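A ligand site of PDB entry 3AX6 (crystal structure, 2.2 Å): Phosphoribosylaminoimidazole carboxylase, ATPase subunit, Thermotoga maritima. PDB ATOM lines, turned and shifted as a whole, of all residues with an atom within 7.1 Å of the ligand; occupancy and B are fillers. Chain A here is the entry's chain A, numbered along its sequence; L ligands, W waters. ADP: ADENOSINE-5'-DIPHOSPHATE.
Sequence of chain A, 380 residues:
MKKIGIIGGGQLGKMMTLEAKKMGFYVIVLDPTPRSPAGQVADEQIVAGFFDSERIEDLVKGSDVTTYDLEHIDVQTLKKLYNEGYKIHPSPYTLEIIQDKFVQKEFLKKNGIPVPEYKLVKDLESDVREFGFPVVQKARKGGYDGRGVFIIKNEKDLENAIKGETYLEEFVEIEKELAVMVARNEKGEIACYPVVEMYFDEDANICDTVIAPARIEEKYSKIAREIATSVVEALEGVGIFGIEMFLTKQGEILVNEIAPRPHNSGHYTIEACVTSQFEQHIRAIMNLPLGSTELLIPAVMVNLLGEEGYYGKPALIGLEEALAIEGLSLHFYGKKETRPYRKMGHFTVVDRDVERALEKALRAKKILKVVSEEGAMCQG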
ATOM      1  N   LYS A 101     -12.924  23.696  29.697  1.00  0.00           N
ATOM      2  CA  LYS A 101     -11.759  22.845  29.587  1.00  0.00           C
ATOM      3  C   LYS A 101     -10.785  22.935  30.744  1.00  0.00           C
ATOM      4  O   LYS A 101     -10.160  21.941  31.100  1.00  0.00           O
ATOM      5  CB  LYS A 101     -11.024  23.123  28.277  1.00  0.00           C
ATOM      6  CG  LYS A 101     -11.800  22.725  27.034  1.00  0.00           C
ATOM      7  CD  LYS A 101     -10.870  22.642  25.830  1.00  0.00           C
ATOM      8  CE  LYS A 101     -11.594  22.075  24.623  1.00  0.00           C
ATOM      9  NZ  LYS A 101     -10.636  21.820  23.509  1.00  0.00           N
ATOM     10  N   LYS A 105      -9.891  19.946  33.258  1.00  0.00           N
ATOM     11  CA  LYS A 105      -8.519  19.472  33.494  1.00  0.00           C
ATOM     12  C   LYS A 105      -8.213  19.437  34.999  1.00  0.00           C
ATOM     13  O   LYS A 105      -7.579  18.508  35.501  1.00  0.00           O
ATOM     14  CB  LYS A 105      -7.515  20.394  32.795  1.00  0.00           C
ATOM     15  CG  LYS A 105      -7.512  20.308  31.277  1.00  0.00           C
ATOM     16  CD  LYS A 105      -7.136  18.916  30.810  1.00  0.00           C
ATOM     17  CE  LYS A 105      -7.155  18.795  29.297  1.00  0.00           C
ATOM     18  NZ  LYS A 105      -6.845  17.404  28.858  1.00  0.00           N
ATOM     19  N   PRO A 116      -2.384  15.647  30.127  1.00  0.00           N
ATOM     20  CA  PRO A 116      -1.197  16.433  29.805  1.00  0.00           C
ATOM     21  C   PRO A 116      -0.982  17.561  30.831  1.00  0.00           C
ATOM     22  O   PRO A 116      -1.941  18.078  31.396  1.00  0.00           O
ATOM     23  CB  PRO A 116      -1.517  16.997  28.430  1.00  0.00           C
ATOM     24  CG  PRO A 116      -2.390  15.943  27.823  1.00  0.00           C
ATOM     25  CD  PRO A 116      -3.296  15.582  28.968  1.00  0.00           C
ATOM     26  N   GLU A 117       0.277  17.932  31.067  1.00  0.00           N
ATOM     27  CA  GLU A 117       0.591  19.020  32.003  1.00  0.00           C
ATOM     28  C   GLU A 117      -0.055  20.289  31.446  1.00  0.00           C
ATOM     29  O   GLU A 117       0.073  20.572  30.264  1.00  0.00           O
ATOM     30  CB  GLU A 117       2.102  19.242  32.093  1.00  0.00           C
ATOM     31  CG  GLU A 117       2.649  19.226  33.497  1.00  0.00           C
ATOM     32  CD  GLU A 117       3.260  17.890  33.865  1.00  0.00           C
ATOM     33  OE1 GLU A 117       4.244  17.488  33.193  1.00  0.00           O
ATOM     34  OE2 GLU A 117       2.762  17.249  34.805  1.00  0.00           O
ATOM     35  N   VAL A 136       0.761  24.190  23.450  1.00  0.00           N
ATOM     36  CA  VAL A 136      -0.601  24.239  22.944  1.00  0.00           C
ATOM     37  C   VAL A 136      -1.517  25.113  23.781  1.00  0.00           C
ATOM     38  O   VAL A 136      -1.597  24.967  25.001  1.00  0.00           O
ATOM     39  CB  VAL A 136      -1.204  22.826  22.871  1.00  0.00           C
ATOM     40  CG1 VAL A 136      -2.540  22.870  22.157  1.00  0.00           C
ATOM     41  CG2 VAL A 136      -0.251  21.887  22.176  1.00  0.00           C
ATOM     42  N   LYS A 138      -5.446  26.519  24.411  1.00  0.00           N
ATOM     43  CA  LYS A 138      -6.831  26.124  24.205  1.00  0.00           C
ATOM     44  C   LYS A 138      -7.788  27.086  24.872  1.00  0.00           C
ATOM     45  O   LYS A 138      -7.544  27.537  25.986  1.00  0.00           O
ATOM     46  CB  LYS A 138      -7.068  24.715  24.752  1.00  0.00           C
ATOM     47  CG  LYS A 138      -6.279  23.636  24.056  1.00  0.00           C
ATOM     48  CD  LYS A 138      -6.610  22.267  24.615  1.00  0.00           C
ATOM     49  CE  LYS A 138      -6.104  21.179  23.690  1.00  0.00           C
ATOM     50  NZ  LYS A 138      -6.439  19.823  24.186  1.00  0.00           N
ATOM     51  N   GLY A 148     -10.197  27.510  18.319  1.00  0.00           N
ATOM     52  CA  GLY A 148     -10.315  26.454  19.313  1.00  0.00           C
ATOM     53  C   GLY A 148      -8.983  26.021  19.921  1.00  0.00           C
ATOM     54  O   GLY A 148      -8.774  26.145  21.124  1.00  0.00           O
ATOM     55  N   VAL A 149      -8.081  25.517  19.076  1.00  0.00           N
ATOM     56  CA  VAL A 149      -6.766  25.084  19.538  1.00  0.00           C
ATOM     57  C   VAL A 149      -5.668  25.742  18.705  1.00  0.00           C
ATOM     58  O   VAL A 149      -5.720  25.754  17.471  1.00  0.00           O
ATOM     59  CB  VAL A 149      -6.596  23.549  19.439  1.00  0.00           C
ATOM     60  CG1 VAL A 149      -6.686  23.099  17.985  1.00  0.00           C
ATOM     61  CG2 VAL A 149      -5.266  23.145  20.040  1.00  0.00           C
ATOM     62  N   ILE A 151      -1.334  26.099  18.325  1.00  0.00           N
ATOM     63  CA  ILE A 151      -0.011  25.636  18.715  1.00  0.00           C
ATOM     64  C   ILE A 151       0.982  26.791  18.593  1.00  0.00           C
ATOM     65  O   ILE A 151       1.306  27.235  17.487  1.00  0.00           O
ATOM     66  CB  ILE A 151       0.433  24.462  17.828  1.00  0.00           C
ATOM     67  CG1 ILE A 151      -0.597  23.334  17.914  1.00  0.00           C
ATOM     68  CG2 ILE A 151       1.795  23.964  18.274  1.00  0.00           C
ATOM     69  CD1 ILE A 151      -0.344  22.183  16.958  1.00  0.00           C
ATOM     70  N   TYR A 167      -6.060  28.410  28.367  1.00  0.00           N
ATOM     71  CA  TYR A 167      -5.116  27.772  29.260  1.00  0.00           C
ATOM     72  C   TYR A 167      -4.085  27.134  28.345  1.00  0.00           C
ATOM     73  O   TYR A 167      -4.289  27.045  27.133  1.00  0.00           O
ATOM     74  CB  TYR A 167      -5.792  26.718  30.154  1.00  0.00           C
ATOM     75  CG  TYR A 167      -6.318  25.492  29.446  1.00  0.00           C
ATOM     76  CD1 TYR A 167      -7.483  25.540  28.681  1.00  0.00           C
ATOM     77  CD2 TYR A 167      -5.652  24.268  29.562  1.00  0.00           C
ATOM     78  CE1 TYR A 167      -7.975  24.399  28.033  1.00  0.00           C
ATOM     79  CE2 TYR A 167      -6.133  23.120  28.920  1.00  0.00           C
ATOM     80  CZ  TYR A 167      -7.297  23.196  28.158  1.00  0.00           C
ATOM     81  OH  TYR A 167      -7.764  22.052  27.532  1.00  0.00           O
ATOM     82  N   GLU A 169      -1.180  23.852  27.640  1.00  0.00           N
ATOM     83  CA  GLU A 169      -0.858  22.471  27.963  1.00  0.00           C
ATOM     84  C   GLU A 169       0.312  22.027  27.098  1.00  0.00           C
ATOM     85  O   GLU A 169       0.522  22.541  25.994  1.00  0.00           O
ATOM     86  CB  GLU A 169      -2.069  21.535  27.820  1.00  0.00           C
ATOM     87  CG  GLU A 169      -2.633  21.302  26.439  1.00  0.00           C
ATOM     88  CD  GLU A 169      -3.813  20.334  26.476  1.00  0.00           C
ATOM     89  OE1 GLU A 169      -4.772  20.593  27.231  1.00  0.00           O
ATOM     90  OE2 GLU A 169      -3.786  19.309  25.762  1.00  0.00           O
ATOM     91  N   GLU A 170       1.101  21.096  27.620  1.00  0.00           N
ATOM     92  CA  GLU A 170       2.270  20.602  26.914  1.00  0.00           C
ATOM     93  C   GLU A 170       1.906  19.934  25.597  1.00  0.00           C
ATOM     94  O   GLU A 170       0.828  19.345  25.468  1.00  0.00           O
ATOM     95  CB  GLU A 170       3.038  19.618  27.801  1.00  0.00           C
ATOM     96  CG  GLU A 170       2.276  18.325  28.071  1.00  0.00           C
ATOM     97  CD  GLU A 170       3.120  17.332  28.848  1.00  0.00           C
ATOM     98  OE1 GLU A 170       4.252  17.058  28.410  1.00  0.00           O
ATOM     99  OE2 GLU A 170       2.638  16.823  29.893  1.00  0.00           O
ATOM    100  N   PHE A 171       2.812  20.023  24.641  1.00  0.00           N
ATOM    101  CA  PHE A 171       2.592  19.418  23.335  1.00  0.00           C
ATOM    102  C   PHE A 171       2.788  17.911  23.458  1.00  0.00           C
ATOM    103  O   PHE A 171       3.835  17.455  23.922  1.00  0.00           O
ATOM    104  CB  PHE A 171       3.570  19.958  22.299  1.00  0.00           C
ATOM    105  CG  PHE A 171       3.319  19.446  20.919  1.00  0.00           C
ATOM    106  CD1 PHE A 171       2.302  19.992  20.145  1.00  0.00           C
ATOM    107  CD2 PHE A 171       4.051  18.381  20.412  1.00  0.00           C
ATOM    108  CE1 PHE A 171       2.021  19.471  18.875  1.00  0.00           C
ATOM    109  CE2 PHE A 171       3.787  17.859  19.146  1.00  0.00           C
ATOM    110  CZ  PHE A 171       2.757  18.405  18.378  1.00  0.00           C
ATOM    111  N   VAL A 172       1.790  17.153  23.035  1.00  0.00           N
ATOM    112  CA  VAL A 172       1.824  15.703  23.102  1.00  0.00           C
ATOM    113  C   VAL A 172       2.089  15.072  21.728  1.00  0.00           C
ATOM    114  O   VAL A 172       1.455  15.447  20.739  1.00  0.00           O
ATOM    115  CB  VAL A 172       0.465  15.154  23.644  1.00  0.00           C
ATOM    116  CG1 VAL A 172       0.375  13.655  23.441  1.00  0.00           C
ATOM    117  CG2 VAL A 172       0.311  15.507  25.125  1.00  0.00           C
ATOM    118  N   GLU A 173       3.031  14.141  21.672  1.00  0.00           N
ATOM    119  CA  GLU A 173       3.339  13.462  20.416  1.00  0.00           C
ATOM    120  C   GLU A 173       2.375  12.297  20.317  1.00  0.00           C
ATOM    121  O   GLU A 173       2.632  11.200  20.841  1.00  0.00           O
ATOM    122  CB  GLU A 173       4.783  12.952  20.389  1.00  0.00           C
ATOM    123  CG  GLU A 173       5.811  14.056  20.585  1.00  0.00           C
ATOM    124  CD  GLU A 173       7.215  13.632  20.157  1.00  0.00           C
ATOM    125  OE1 GLU A 173       7.648  12.513  20.516  1.00  0.00           O
ATOM    126  OE2 GLU A 173       7.879  14.428  19.458  1.00  0.00           O
ATOM    127  N   ILE A 174       1.257  12.540  19.641  1.00  0.00           N
ATOM    128  CA  ILE A 174       0.205  11.550  19.457  1.00  0.00           C
ATOM    129  C   ILE A 174       0.545  10.448  18.469  1.00  0.00           C
ATOM    130  O   ILE A 174       0.982  10.723  17.362  1.00  0.00           O
ATOM    131  CB  ILE A 174      -1.114  12.252  19.015  1.00  0.00           C
ATOM    132  CG1 ILE A 174      -1.537  13.260  20.083  1.00  0.00           C
ATOM    133  CG2 ILE A 174      -2.222  11.216  18.828  1.00  0.00           C
ATOM    134  CD1 ILE A 174      -2.697  14.129  19.668  1.00  0.00           C
ATOM    135  N   GLU A 177      -5.292   8.414  18.170  1.00  0.00           N
ATOM    136  CA  GLU A 177      -6.300   9.105  18.960  1.00  0.00           C
ATOM    137  C   GLU A 177      -7.423   8.106  19.166  1.00  0.00           C
ATOM    138  O   GLU A 177      -7.956   7.556  18.207  1.00  0.00           O
ATOM    139  CB  GLU A 177      -6.769  10.380  18.240  1.00  0.00           C
ATOM    140  CG  GLU A 177      -5.701  11.481  18.277  1.00  0.00           C
ATOM    141  CD  GLU A 177      -6.201  12.834  17.808  1.00  0.00           C
ATOM    142  OE1 GLU A 177      -7.259  13.269  18.308  1.00  0.00           O
ATOM    143  OE2 GLU A 177      -5.516  13.479  16.964  1.00  0.00           O
ATOM    144  N   GLU A 244     -12.517  10.825  25.049  1.00  0.00           N
ATOM    145  CA  GLU A 244     -11.493  10.901  24.008  1.00  0.00           C
ATOM    146  C   GLU A 244     -10.117  10.905  24.634  1.00  0.00           C
ATOM    147  O   GLU A 244      -9.842  11.678  25.542  1.00  0.00           O
ATOM    148  CB  GLU A 244     -11.712  12.146  23.156  1.00  0.00           C
ATOM    149  CG  GLU A 244     -13.050  12.126  22.458  1.00  0.00           C
ATOM    150  CD  GLU A 244     -13.405  13.469  21.861  1.00  0.00           C
ATOM    151  OE1 GLU A 244     -12.544  14.062  21.176  1.00  0.00           O
ATOM    152  OE2 GLU A 244     -14.550  13.933  22.084  1.00  0.00           O
ATOM    153  N   PHE A 246      -5.571  10.156  24.097  1.00  0.00           N
ATOM    154  CA  PHE A 246      -4.405  10.147  23.227  1.00  0.00           C
ATOM    155  C   PHE A 246      -3.486   9.006  23.627  1.00  0.00           C
ATOM    156  O   PHE A 246      -3.257   8.776  24.816  1.00  0.00           O
ATOM    157  CB  PHE A 246      -3.567  11.421  23.370  1.00  0.00           C
ATOM    158  CG  PHE A 246      -4.243  12.670  22.889  1.00  0.00           C
ATOM    159  CD1 PHE A 246      -5.144  12.639  21.827  1.00  0.00           C
ATOM    160  CD2 PHE A 246      -3.940  13.890  23.472  1.00  0.00           C
ATOM    161  CE1 PHE A 246      -5.732  13.805  21.354  1.00  0.00           C
ATOM    162  CE2 PHE A 246      -4.517  15.076  23.008  1.00  0.00           C
ATOM    163  CZ  PHE A 246      -5.412  15.023  21.942  1.00  0.00           C
ATOM    164  N   LEU A 254      -3.514   9.402  27.683  1.00  0.00           N
ATOM    165  CA  LEU A 254      -4.003  10.605  28.340  1.00  0.00           C
ATOM    166  C   LEU A 254      -5.412  10.958  27.877  1.00  0.00           C
ATOM    167  O   LEU A 254      -5.745  10.780  26.710  1.00  0.00           O
ATOM    168  CB  LEU A 254      -3.062  11.780  28.024  1.00  0.00           C
ATOM    169  CG  LEU A 254      -1.616  11.796  28.545  1.00  0.00           C
ATOM    170  CD1 LEU A 254      -0.974  10.450  28.375  1.00  0.00           C
ATOM    171  CD2 LEU A 254      -0.798  12.850  27.820  1.00  0.00           C
ATOM    172  N   ASN A 256      -8.093  13.557  26.772  1.00  0.00           N
ATOM    173  CA  ASN A 256      -8.158  14.897  26.204  1.00  0.00           C
ATOM    174  C   ASN A 256      -9.512  15.574  26.310  1.00  0.00           C
ATOM    175  O   ASN A 256      -9.591  16.775  26.595  1.00  0.00           O
ATOM    176  CB  ASN A 256      -7.737  14.829  24.727  1.00  0.00           C
ATOM    177  CG  ASN A 256      -8.043  16.099  23.959  1.00  0.00           C
ATOM    178  OD1 ASN A 256      -7.586  17.174  24.330  1.00  0.00           O
ATOM    179  ND2 ASN A 256      -8.812  15.977  22.886  1.00  0.00           N
ATOM    180  N   GLU A 257     -10.586  14.814  26.105  1.00  0.00           N
ATOM    181  CA  GLU A 257     -11.919  15.404  26.138  1.00  0.00           C
ATOM    182  C   GLU A 257     -12.999  14.459  26.660  1.00  0.00           C
ATOM    183  O   GLU A 257     -12.875  13.245  26.571  1.00  0.00           O
ATOM    184  CB  GLU A 257     -12.285  15.874  24.729  1.00  0.00           C
ATOM    185  CG  GLU A 257     -13.545  16.713  24.638  1.00  0.00           C
ATOM    186  CD  GLU A 257     -13.394  18.044  25.331  1.00  0.00           C
ATOM    187  OE1 GLU A 257     -12.664  18.905  24.819  1.00  0.00           O
ATOM    188  OE2 GLU A 257     -14.014  18.223  26.392  1.00  0.00           O
HETATM  189  PB  ADP L   1     -11.535  20.346  19.709  1.00  0.00           P
HETATM  190  O1B ADP L   1     -11.961  18.921  19.833  1.00  0.00           O
HETATM  191  O2B ADP L   1     -11.382  20.713  18.132  1.00  0.00           O
HETATM  192  O3B ADP L   1     -12.708  21.322  20.426  1.00  0.00           O
HETATM  193  PA  ADP L   1      -9.114  19.351  20.665  1.00  0.00           P
HETATM  194  O1A ADP L   1      -8.691  19.304  22.085  1.00  0.00           O
HETATM  195  O2A ADP L   1      -9.830  17.942  20.291  1.00  0.00           O
HETATM  196  O3A ADP L   1     -10.113  20.648  20.469  1.00  0.00           O
HETATM  197  O5' ADP L   1      -7.796  19.608  19.748  1.00  0.00           O
HETATM  198  C5' ADP L   1      -8.037  19.090  18.427  1.00  0.00           C
HETATM  199  C4' ADP L   1      -6.793  18.364  17.904  1.00  0.00           C
HETATM  200  O4' ADP L   1      -5.569  19.087  18.280  1.00  0.00           O
HETATM  201  C3' ADP L   1      -6.666  16.955  18.493  1.00  0.00           C
HETATM  202  O3' ADP L   1      -7.401  15.978  17.737  1.00  0.00           O
HETATM  203  C2' ADP L   1      -5.159  16.717  18.479  1.00  0.00           C
HETATM  204  O2' ADP L   1      -4.725  16.137  17.246  1.00  0.00           O
HETATM  205  C1' ADP L   1      -4.563  18.116  18.717  1.00  0.00           C
HETATM  206  N9  ADP L   1      -4.193  18.321  20.133  1.00  0.00           N
HETATM  207  C8  ADP L   1      -5.023  18.617  21.187  1.00  0.00           C
HETATM  208  N7  ADP L   1      -4.343  18.720  22.285  1.00  0.00           N
HETATM  209  C5  ADP L   1      -3.039  18.493  22.031  1.00  0.00           C
HETATM  210  C6  ADP L   1      -1.845  18.464  22.808  1.00  0.00           C
HETATM  211  N6  ADP L   1      -1.892  18.701  24.165  1.00  0.00           N
HETATM  212  N1  ADP L   1      -0.670  18.196  22.200  1.00  0.00           N
HETATM  213  C2  ADP L   1      -0.597  17.960  20.886  1.00  0.00           C
HETATM  214  N3  ADP L   1      -1.694  17.983  20.122  1.00  0.00           N
HETATM  215  C4  ADP L   1      -2.915  18.240  20.639  1.00  0.00           C
HETATM  216  O   HOH W   1      -7.393  21.102  15.652  1.00  0.00           O
HETATM  217  O   HOH W   2      -4.145  20.888  16.472  1.00  0.00           O
HETATM  218  O   HOH W   3      -9.925  14.489  20.815  1.00  0.00           O
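Water W3 lies within hydrogen-bond range of OE1 of Glu 244, ND2 of Asn 256 and O2A of the ligand.
OE2 of Glu 169 lies within hydrogen-bond range of N6 of the ligand. NZ of Lys 138 lies within salt-bridge range of O1A of the ligand, 3.1 Å away. An oxygen (O1A) of the ligand lies within salt-bridge range of the side-chain amino group (NZ) of Lys 101, at 3.5 Å. OD1 of Asn 256 sits close to O1A of the ligand (3.3 Å). O3' of the ligand lies within hydrogen-bond range of OE1 of Glu 177. N of Val 172 is in hydrogen-bond range of N1 of the ligand (2.8 Å). O of Glu 170 sits at hydrogen-bond distance from N6 of the ligand (3.1 Å).
The side-chain amino group (NZ) of Lys 101 is in salt-bridge range of the side-chain carboxylate (OE1) of Glu 257 (3.8 Å). OE2 of Glu 170 lies within hydrogen-bond range of N of Glu 117 (2.9 Å). The side-chain amino group (NZ) of Lys 138 is in hydrogen-bond range of the side-chain amide oxygen (OD1) of Asn 256, at 2.9 Å. N of Tyr 167 is in hydrogen-bond range of O of Lys 138 (2.9 Å). OE1 of Glu 169 lies close to OH of Tyr 167. N of Phe 246 sits at hydrogen-bond distance from O of Leu 254 (2.7 Å). The backbone NH (N) of Asn 256 lies within hydrogen-bond range of the backbone carbonyl oxygen (O) of Glu 244 (2.8 Å). OE2 of Glu 169 is in salt-bridge range of NZ of Lys 138.
CG2 of Val 136 touches N1 of the ligand, at 3.7 Å. CD1 of Phe 171 touches C2 of the ligand, at 3.6 Å. Ile 174 touches the ligand (CD1 to O2', 3.7 Å). Phe 246 touches the ligand (CZ to C8, 3.7 Å). Hydrophobic or aromatic side chains that line the ligand: Val 136, Phe 171, Val 172, Ile 174 and Phe 246. The nearest printed residue that does not touch the ligand is Val 149 (4.1 Å).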
